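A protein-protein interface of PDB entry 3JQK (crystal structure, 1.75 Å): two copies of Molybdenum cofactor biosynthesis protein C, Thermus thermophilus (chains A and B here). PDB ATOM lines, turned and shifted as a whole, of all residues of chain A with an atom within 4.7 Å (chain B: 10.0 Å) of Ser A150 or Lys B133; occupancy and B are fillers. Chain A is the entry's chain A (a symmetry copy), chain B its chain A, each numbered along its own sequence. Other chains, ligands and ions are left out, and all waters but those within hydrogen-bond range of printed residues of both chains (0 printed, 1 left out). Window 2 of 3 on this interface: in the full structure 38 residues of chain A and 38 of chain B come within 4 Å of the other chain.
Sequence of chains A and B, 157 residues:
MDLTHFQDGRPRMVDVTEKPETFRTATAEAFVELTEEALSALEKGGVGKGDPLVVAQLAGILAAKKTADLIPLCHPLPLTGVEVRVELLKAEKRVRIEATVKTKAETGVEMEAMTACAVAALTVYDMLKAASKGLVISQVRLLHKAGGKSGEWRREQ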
ATOM      1  N   GLU A 110     -10.742 -27.256  12.531  1.00  0.00           N
ATOM      2  CA  GLU A 110      -9.999 -26.287  13.316  1.00  0.00           C
ATOM      3  C   GLU A 110      -9.670 -26.892  14.670  1.00  0.00           C
ATOM      4  O   GLU A 110      -8.566 -26.717  15.177  1.00  0.00           O
ATOM      5  CB  GLU A 110     -10.807 -25.005  13.516  1.00  0.00           C
ATOM      6  CG  GLU A 110     -11.123 -24.283  12.223  1.00  0.00           C
ATOM      7  CD  GLU A 110     -12.495 -24.615  11.681  1.00  0.00           C
ATOM      8  OE1 GLU A 110     -12.963 -25.760  11.860  1.00  0.00           O
ATOM      9  OE2 GLU A 110     -13.104 -23.721  11.060  1.00  0.00           O
ATOM     10  N   LEU A 142      -5.284 -20.357  15.863  1.00  0.00           N
ATOM     11  CA  LEU A 142      -5.531 -20.800  14.497  1.00  0.00           C
ATOM     12  C   LEU A 142      -4.828 -19.846  13.540  1.00  0.00           C
ATOM     13  O   LEU A 142      -4.857 -18.623  13.732  1.00  0.00           O
ATOM     14  CB  LEU A 142      -7.034 -20.813  14.208  1.00  0.00           C
ATOM     15  CG  LEU A 142      -7.458 -21.569  12.940  1.00  0.00           C
ATOM     16  CD1 LEU A 142      -7.219 -23.058  13.149  1.00  0.00           C
ATOM     17  CD2 LEU A 142      -8.922 -21.308  12.632  1.00  0.00           C
ATOM     18  N   LYS A 145      -7.614 -21.713   7.693  1.00  0.00           N
ATOM     19  CA  LYS A 145      -8.611 -22.745   7.490  1.00  0.00           C
ATOM     20  C   LYS A 145      -9.277 -22.465   6.153  1.00  0.00           C
ATOM     21  O   LYS A 145      -9.306 -21.320   5.691  1.00  0.00           O
ATOM     22  CB  LYS A 145      -9.642 -22.758   8.631  1.00  0.00           C
ATOM     23  CG  LYS A 145     -10.731 -21.687   8.581  1.00  0.00           C
ATOM     24  CD  LYS A 145     -11.877 -22.086   7.652  1.00  0.00           C
ATOM     25  CE  LYS A 145     -13.044 -21.121   7.779  1.00  0.00           C
ATOM     26  NZ  LYS A 145     -14.188 -21.518   6.906  1.00  0.00           N
ATOM     27  N   GLY A 147     -12.596 -24.138   3.367  1.00  0.00           N
ATOM     28  CA  GLY A 147     -13.751 -25.007   3.275  1.00  0.00           C
ATOM     29  C   GLY A 147     -14.866 -24.439   4.132  1.00  0.00           C
ATOM     30  O   GLY A 147     -14.603 -23.679   5.065  1.00  0.00           O
ATOM     31  N   GLY A 148     -16.107 -24.801   3.820  1.00  0.00           N
ATOM     32  CA  GLY A 148     -17.240 -24.302   4.580  1.00  0.00           C
ATOM     33  C   GLY A 148     -17.816 -23.021   4.001  1.00  0.00           C
ATOM     34  O   GLY A 148     -17.218 -22.409   3.116  1.00  0.00           O
ATOM     35  N   LYS A 149     -18.981 -22.617   4.504  1.00  0.00           N
ATOM     36  CA  LYS A 149     -19.651 -21.402   4.044  1.00  0.00           C
ATOM     37  C   LYS A 149     -18.734 -20.182   4.118  1.00  0.00           C
ATOM     38  O   LYS A 149     -18.500 -19.510   3.113  1.00  0.00           O
ATOM     39  CB  LYS A 149     -20.904 -21.140   4.889  1.00  0.00           C
ATOM     40  CG  LYS A 149     -21.549 -19.777   4.649  1.00  0.00           C
ATOM     41  CD  LYS A 149     -22.527 -19.796   3.485  1.00  0.00           C
ATOM     42  CE  LYS A 149     -23.929 -20.163   3.948  1.00  0.00           C
ATOM     43  NZ  LYS A 149     -24.493 -19.135   4.873  1.00  0.00           N
ATOM     44  N   SER A 150     -18.220 -19.908   5.315  1.00  0.00           N
ATOM     45  CA  SER A 150     -17.341 -18.765   5.543  1.00  0.00           C
ATOM     46  C   SER A 150     -16.151 -18.698   4.588  1.00  0.00           C
ATOM     47  O   SER A 150     -15.560 -17.635   4.402  1.00  0.00           O
ATOM     48  CB  SER A 150     -16.847 -18.764   6.995  1.00  0.00           C
ATOM     49  OG  SER A 150     -16.281 -20.013   7.352  1.00  0.00           O
ATOM     50  N   GLY A 151     -15.802 -19.829   3.984  1.00  0.00           N
ATOM     51  CA  GLY A 151     -14.690 -19.853   3.050  1.00  0.00           C
ATOM     52  C   GLY A 151     -13.318 -19.817   3.699  1.00  0.00           C
ATOM     53  O   GLY A 151     -13.159 -20.199   4.858  1.00  0.00           O
ATOM     54  N   GLU A 152     -12.325 -19.349   2.948  1.00  0.00           N
ATOM     55  CA  GLU A 152     -10.959 -19.274   3.445  1.00  0.00           C
ATOM     56  C   GLU A 152     -10.783 -18.171   4.487  1.00  0.00           C
ATOM     57  O   GLU A 152     -11.342 -17.081   4.360  1.00  0.00           O
ATOM     58  CB  GLU A 152      -9.990 -19.051   2.282  1.00  0.00           C
ATOM     59  CG  GLU A 152      -8.550 -19.360   2.630  1.00  0.00           C
ATOM     60  CD  GLU A 152      -7.867 -20.187   1.563  1.00  0.00           C
ATOM     61  OE1 GLU A 152      -8.581 -20.842   0.772  1.00  0.00           O
ATOM     62  OE2 GLU A 152      -6.621 -20.199   1.521  1.00  0.00           O
ATOM     63  N   TRP A 153     -10.001 -18.474   5.520  1.00  0.00           N
ATOM     64  CA  TRP A 153      -9.724 -17.539   6.609  1.00  0.00           C
ATOM     65  C   TRP A 153      -8.245 -17.583   6.958  1.00  0.00           C
ATOM     66  O   TRP A 153      -7.649 -18.655   7.010  1.00  0.00           O
ATOM     67  CB  TRP A 153     -10.526 -17.920   7.854  1.00  0.00           C
ATOM     68  CG  TRP A 153     -10.253 -17.031   9.044  1.00  0.00           C
ATOM     69  CD1 TRP A 153     -10.910 -15.880   9.374  1.00  0.00           C
ATOM     70  CD2 TRP A 153      -9.245 -17.218  10.049  1.00  0.00           C
ATOM     71  NE1 TRP A 153     -10.377 -15.341  10.522  1.00  0.00           N
ATOM     72  CE2 TRP A 153      -9.352 -16.141  10.956  1.00  0.00           C
ATOM     73  CE3 TRP A 153      -8.260 -18.190  10.270  1.00  0.00           C
ATOM     74  CZ2 TRP A 153      -8.514 -16.009  12.071  1.00  0.00           C
ATOM     75  CZ3 TRP A 153      -7.425 -18.061  11.378  1.00  0.00           C
ATOM     76  CH2 TRP A 153      -7.560 -16.977  12.264  1.00  0.00           C
ATOM     77  N   VAL B  32      -8.223 -17.563  27.842  1.00  0.00           N
ATOM     78  CA  VAL B  32      -8.693 -17.425  26.473  1.00  0.00           C
ATOM     79  C   VAL B  32      -8.989 -15.930  26.345  1.00  0.00           C
ATOM     80  O   VAL B  32      -9.819 -15.391  27.090  1.00  0.00           O
ATOM     81  CB  VAL B  32      -9.984 -18.227  26.203  1.00  0.00           C
ATOM     82  CG1 VAL B  32     -10.412 -18.021  24.760  1.00  0.00           C
ATOM     83  CG2 VAL B  32      -9.743 -19.711  26.479  1.00  0.00           C
ATOM     84  N   GLU B  33      -8.284 -15.256  25.438  1.00  0.00           N
ATOM     85  CA  GLU B  33      -8.475 -13.820  25.230  1.00  0.00           C
ATOM     86  C   GLU B  33      -9.663 -13.600  24.300  1.00  0.00           C
ATOM     87  O   GLU B  33      -9.693 -14.124  23.187  1.00  0.00           O
ATOM     88  CB  GLU B  33      -7.210 -13.200  24.631  1.00  0.00           C
ATOM     89  CG  GLU B  33      -5.936 -13.458  25.438  1.00  0.00           C
ATOM     90  CD  GLU B  33      -6.084 -13.120  26.915  1.00  0.00           C
ATOM     91  OE1 GLU B  33      -6.624 -12.041  27.244  1.00  0.00           O
ATOM     92  OE2 GLU B  33      -5.646 -13.935  27.757  1.00  0.00           O
ATOM     93  N   THR B  35     -12.616 -11.308  22.051  1.00  0.00           N
ATOM     94  CA  THR B  35     -12.830 -10.129  21.218  1.00  0.00           C
ATOM     95  C   THR B  35     -14.174  -9.622  21.732  1.00  0.00           C
ATOM     96  O   THR B  35     -14.827 -10.313  22.508  1.00  0.00           O
ATOM     97  CB  THR B  35     -12.967 -10.487  19.719  1.00  0.00           C
ATOM     98  OG1 THR B  35     -13.935 -11.533  19.565  1.00  0.00           O
ATOM     99  CG2 THR B  35     -11.631 -10.935  19.145  1.00  0.00           C
ATOM    100  N   GLU B  37     -16.837  -9.381  20.102  1.00  0.00           N
ATOM    101  CA  GLU B  37     -17.829 -10.292  19.543  1.00  0.00           C
ATOM    102  C   GLU B  37     -18.004 -11.524  20.419  1.00  0.00           C
ATOM    103  O   GLU B  37     -19.121 -11.918  20.724  1.00  0.00           O
ATOM    104  CB  GLU B  37     -17.432 -10.746  18.130  1.00  0.00           C
ATOM    105  CG  GLU B  37     -17.201  -9.643  17.112  1.00  0.00           C
ATOM    106  CD  GLU B  37     -15.738  -9.232  16.997  1.00  0.00           C
ATOM    107  OE1 GLU B  37     -15.198  -8.613  17.942  1.00  0.00           O
ATOM    108  OE2 GLU B  37     -15.122  -9.522  15.949  1.00  0.00           O
ATOM    109  N   ALA B  38     -16.890 -12.138  20.803  1.00  0.00           N
ATOM    110  CA  ALA B  38     -16.918 -13.335  21.644  1.00  0.00           C
ATOM    111  C   ALA B  38     -17.466 -13.026  23.042  1.00  0.00           C
ATOM    112  O   ALA B  38     -18.229 -13.815  23.610  1.00  0.00           O
ATOM    113  CB  ALA B  38     -15.517 -13.932  21.754  1.00  0.00           C
ATOM    114  N   VAL B 124     -13.703 -23.952  25.151  1.00  0.00           N
ATOM    115  CA  VAL B 124     -14.237 -22.598  25.100  1.00  0.00           C
ATOM    116  C   VAL B 124     -14.052 -22.111  23.661  1.00  0.00           C
ATOM    117  O   VAL B 124     -14.953 -21.514  23.073  1.00  0.00           O
ATOM    118  CB  VAL B 124     -13.474 -21.652  26.053  1.00  0.00           C
ATOM    119  CG1 VAL B 124     -13.860 -20.194  25.769  1.00  0.00           C
ATOM    120  CG2 VAL B 124     -13.794 -22.004  27.495  1.00  0.00           C
ATOM    121  N   TYR B 125     -12.874 -22.374  23.096  1.00  0.00           N
ATOM    122  CA  TYR B 125     -12.592 -21.966  21.724  1.00  0.00           C
ATOM    123  C   TYR B 125     -13.589 -22.630  20.772  1.00  0.00           C
ATOM    124  O   TYR B 125     -14.146 -21.984  19.887  1.00  0.00           O
ATOM    125  CB  TYR B 125     -11.159 -22.360  21.329  1.00  0.00           C
ATOM    126  CG  TYR B 125     -10.830 -22.034  19.889  1.00  0.00           C
ATOM    127  CD1 TYR B 125     -10.506 -20.734  19.503  1.00  0.00           C
ATOM    128  CD2 TYR B 125     -10.900 -23.014  18.901  1.00  0.00           C
ATOM    129  CE1 TYR B 125     -10.262 -20.418  18.159  1.00  0.00           C
ATOM    130  CE2 TYR B 125     -10.659 -22.714  17.563  1.00  0.00           C
ATOM    131  CZ  TYR B 125     -10.344 -21.414  17.198  1.00  0.00           C
ATOM    132  OH  TYR B 125     -10.136 -21.111  15.869  1.00  0.00           O
ATOM    133  N   ASP B 126     -13.825 -23.926  20.961  1.00  0.00           N
ATOM    134  CA  ASP B 126     -14.755 -24.641  20.091  1.00  0.00           C
ATOM    135  C   ASP B 126     -16.144 -24.012  20.087  1.00  0.00           C
ATOM    136  O   ASP B 126     -16.779 -23.903  19.034  1.00  0.00           O
ATOM    137  CB  ASP B 126     -14.882 -26.108  20.521  1.00  0.00           C
ATOM    138  CG  ASP B 126     -15.873 -26.879  19.660  1.00  0.00           C
ATOM    139  OD1 ASP B 126     -15.668 -26.923  18.433  1.00  0.00           O
ATOM    140  OD2 ASP B 126     -16.852 -27.435  20.205  1.00  0.00           O
ATOM    141  N   MET B 127     -16.595 -23.592  21.266  1.00  0.00           N
ATOM    142  CA  MET B 127     -17.922 -23.002  21.448  1.00  0.00           C
ATOM    143  C   MET B 127     -18.048 -21.563  20.945  1.00  0.00           C
ATOM    144  O   MET B 127     -19.161 -21.056  20.805  1.00  0.00           O
ATOM    145  CB  MET B 127     -18.309 -22.998  22.933  1.00  0.00           C
ATOM    146  CG  MET B 127     -17.981 -24.246  23.748  1.00  0.00           C
ATOM    147  SD  MET B 127     -19.259 -25.521  23.807  1.00  0.00           S
ATOM    148  CE  MET B 127     -20.712 -24.583  24.258  1.00  0.00           C
ATOM    149  N   LEU B 128     -16.927 -20.901  20.683  1.00  0.00           N
ATOM    150  CA  LEU B 128     -16.968 -19.507  20.238  1.00  0.00           C
ATOM    151  C   LEU B 128     -16.283 -19.210  18.907  1.00  0.00           C
ATOM    152  O   LEU B 128     -16.327 -18.074  18.430  1.00  0.00           O
ATOM    153  CB  LEU B 128     -16.350 -18.604  21.312  1.00  0.00           C
ATOM    154  CG  LEU B 128     -16.959 -18.598  22.714  1.00  0.00           C
ATOM    155  CD1 LEU B 128     -16.087 -17.753  23.639  1.00  0.00           C
ATOM    156  CD2 LEU B 128     -18.383 -18.048  22.667  1.00  0.00           C
ATOM    157  N   LYS B 129     -15.660 -20.215  18.303  1.00  0.00           N
ATOM    158  CA  LYS B 129     -14.950 -20.013  17.042  1.00  0.00           C
ATOM    159  C   LYS B 129     -15.844 -19.699  15.841  1.00  0.00           C
ATOM    160  O   LYS B 129     -15.376 -19.148  14.842  1.00  0.00           O
ATOM    161  CB  LYS B 129     -14.088 -21.235  16.719  1.00  0.00           C
ATOM    162  CG  LYS B 129     -14.869 -22.474  16.309  1.00  0.00           C
ATOM    163  CD  LYS B 129     -13.921 -23.614  15.978  1.00  0.00           C
ATOM    164  CE  LYS B 129     -14.651 -24.761  15.304  1.00  0.00           C
ATOM    165  NZ  LYS B 129     -15.807 -25.219  16.116  1.00  0.00           N
ATOM    166  N   ALA B 130     -17.121 -20.054  15.932  1.00  0.00           N
ATOM    167  CA  ALA B 130     -18.052 -19.806  14.836  1.00  0.00           C
ATOM    168  C   ALA B 130     -17.992 -18.347  14.400  1.00  0.00           C
ATOM    169  O   ALA B 130     -17.868 -18.044  13.210  1.00  0.00           O
ATOM    170  CB  ALA B 130     -19.470 -20.165  15.263  1.00  0.00           C
ATOM    171  N   ALA B 131     -18.071 -17.446  15.374  1.00  0.00           N
ATOM    172  CA  ALA B 131     -18.030 -16.016  15.102  1.00  0.00           C
ATOM    173  C   ALA B 131     -16.629 -15.424  15.257  1.00  0.00           C
ATOM    174  O   ALA B 131     -16.323 -14.391  14.660  1.00  0.00           O
ATOM    175  CB  ALA B 131     -19.008 -15.289  16.025  1.00  0.00           C
ATOM    176  N   SER B 132     -15.779 -16.074  16.050  1.00  0.00           N
ATOM    177  CA  SER B 132     -14.425 -15.573  16.273  1.00  0.00           C
ATOM    178  C   SER B 132     -13.354 -16.657  16.145  1.00  0.00           C
ATOM    179  O   SER B 132     -12.908 -17.227  17.142  1.00  0.00           O
ATOM    180  CB  SER B 132     -14.337 -14.935  17.660  1.00  0.00           C
ATOM    181  OG  SER B 132     -15.380 -13.996  17.855  1.00  0.00           O
ATOM    182  N   LYS B 133     -12.932 -16.926  14.916  1.00  0.00           N
ATOM    183  CA  LYS B 133     -11.919 -17.944  14.669  1.00  0.00           C
ATOM    184  C   LYS B 133     -10.528 -17.565  15.155  1.00  0.00           C
ATOM    185  O   LYS B 133      -9.682 -18.438  15.353  1.00  0.00           O
ATOM    186  CB  LYS B 133     -11.869 -18.277  13.176  1.00  0.00           C
ATOM    187  CG  LYS B 133     -13.085 -19.045  12.705  1.00  0.00           C
ATOM    188  CD  LYS B 133     -13.144 -19.170  11.199  1.00  0.00           C
ATOM    189  CE  LYS B 133     -14.378 -19.960  10.795  1.00  0.00           C
ATOM    190  NZ  LYS B 133     -15.606 -19.417  11.446  1.00  0.00           N
ATOM    191  N   GLY B 134     -10.298 -16.269  15.362  1.00  0.00           N
ATOM    192  CA  GLY B 134      -8.994 -15.808  15.809  1.00  0.00           C
ATOM    193  C   GLY B 134      -8.724 -15.810  17.303  1.00  0.00           C
ATOM    194  O   GLY B 134      -7.651 -15.381  17.732  1.00  0.00           O
ATOM    195  N   LEU B 135      -9.677 -16.286  18.103  1.00  0.00           N
ATOM    196  CA  LEU B 135      -9.493 -16.329  19.553  1.00  0.00           C
ATOM    197  C   LEU B 135      -8.227 -17.094  19.909  1.00  0.00           C
ATOM    198  O   LEU B 135      -7.939 -18.142  19.330  1.00  0.00           O
ATOM    199  CB  LEU B 135     -10.697 -16.986  20.227  1.00  0.00           C
ATOM    200  CG  LEU B 135     -12.026 -16.235  20.104  1.00  0.00           C
ATOM    201  CD1 LEU B 135     -13.123 -17.021  20.795  1.00  0.00           C
ATOM    202  CD2 LEU B 135     -11.892 -14.852  20.728  1.00  0.00           C
ATOM    203  N   VAL B 136      -7.484 -16.569  20.877  1.00  0.00           N
ATOM    204  CA  VAL B 136      -6.228 -17.172  21.301  1.00  0.00           C
ATOM    205  C   VAL B 136      -6.252 -17.740  22.716  1.00  0.00           C
ATOM    206  O   VAL B 136      -6.822 -17.142  23.628  1.00  0.00           O
ATOM    207  CB  VAL B 136      -5.078 -16.126  21.247  1.00  0.00           C
ATOM    208  CG1 VAL B 136      -3.778 -16.732  21.765  1.00  0.00           C
ATOM    209  CG2 VAL B 136      -4.897 -15.625  19.832  1.00  0.00           C
ATOM    210  N   ILE B 137      -5.650 -18.912  22.886  1.00  0.00           N
ATOM    211  CA  ILE B 137      -5.517 -19.507  24.210  1.00  0.00           C
ATOM    212  C   ILE B 137      -4.138 -18.939  24.539  1.00  0.00           C
ATOM    213  O   ILE B 137      -3.108 -19.457  24.094  1.00  0.00           O
ATOM    214  CB  ILE B 137      -5.502 -21.050  24.144  1.00  0.00           C
ATOM    215  CG1 ILE B 137      -6.898 -21.549  23.748  1.00  0.00           C
ATOM    216  CG2 ILE B 137      -5.093 -21.625  25.495  1.00  0.00           C
ATOM    217  CD1 ILE B 137      -6.975 -23.048  23.453  1.00  0.00           C
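O of Lys B129 sits close to NZ of Lys B133, at 3.4 Å.
The side-chain amino group (NZ) of Lys A145 sits at hydrogen-bond distance from the side-chain hydroxyl (OG) of Ser A150, at 2.6 Å.
The side-chain hydroxyl (OH) of Tyr B125 lies within hydrogen-bond range of the backbone carbonyl oxygen (O) of Lys B133, at 2.8 Å.
The backbone carbonyl oxygen of Gly A151 is in hydrogen-bond range of the side-chain amino group of Lys A145 (2.6 Å).
NZ of Lys A145 lies within hydrogen-bond range of O of Gly A147 (2.9 Å).
NZ of Lys B129 lies within salt-bridge range of OD1 of Asp B126.
Glu A110 touches Lys B129 (OE1 to CE, 3.96 Å).
Lys B133 touches Glu A110.
Tyr B125 touches Leu A142 (OH to CD2, 3.5 Å).
Leu A142 touches Lys B133 (CB to O, 3.7 Å).
CE of Lys B133 touches CE of Lys A145, at 3.5 Å.
Lys B133 touches Ser A150.
Trp A153 touches Lys B133.
N of Gly B134 touches CZ2 of Trp A153, at 3.8 Å.
Printed residues of chain B within 4 Å of Ser A150: Lys B133.
Leu A142 touches two residues of chain B.
No residue of chain B comes within 4 Å of Gly A148.
Of the printed residues of chain A, Lys B129 touches Glu A110.
Of the printed residues of chain A, Gly B134 touches Trp A153 (3.8 Å).
The nearest printed residue of chain A that does not touch Lys B133 is Gly A151 (6.1 Å).
The nearest printed residue of chain A that does not touch Lys B129 is Leu A142 (6.4 Å).
Hydrophobic or aromatic side chains of chain B within 4 Å of the printed part of chain A: Tyr B125.
Of the 10 printed residues of chain A, 5 touch a printed residue of chain B.
Hydrophobic or aromatic side chains of chain A within 4 Å of the printed part of chain B: Leu A142 and Trp A153.
Along chain A the printed residues that touch a printed residue of chain B span positions 110 to 153.
Among the printed residues, 8 pairs touch across the chains.
No position is printed for both chains.
Of the 8 pairs that touch across the chains among the printed residues, none has its exchanged pair printed and touching as well.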
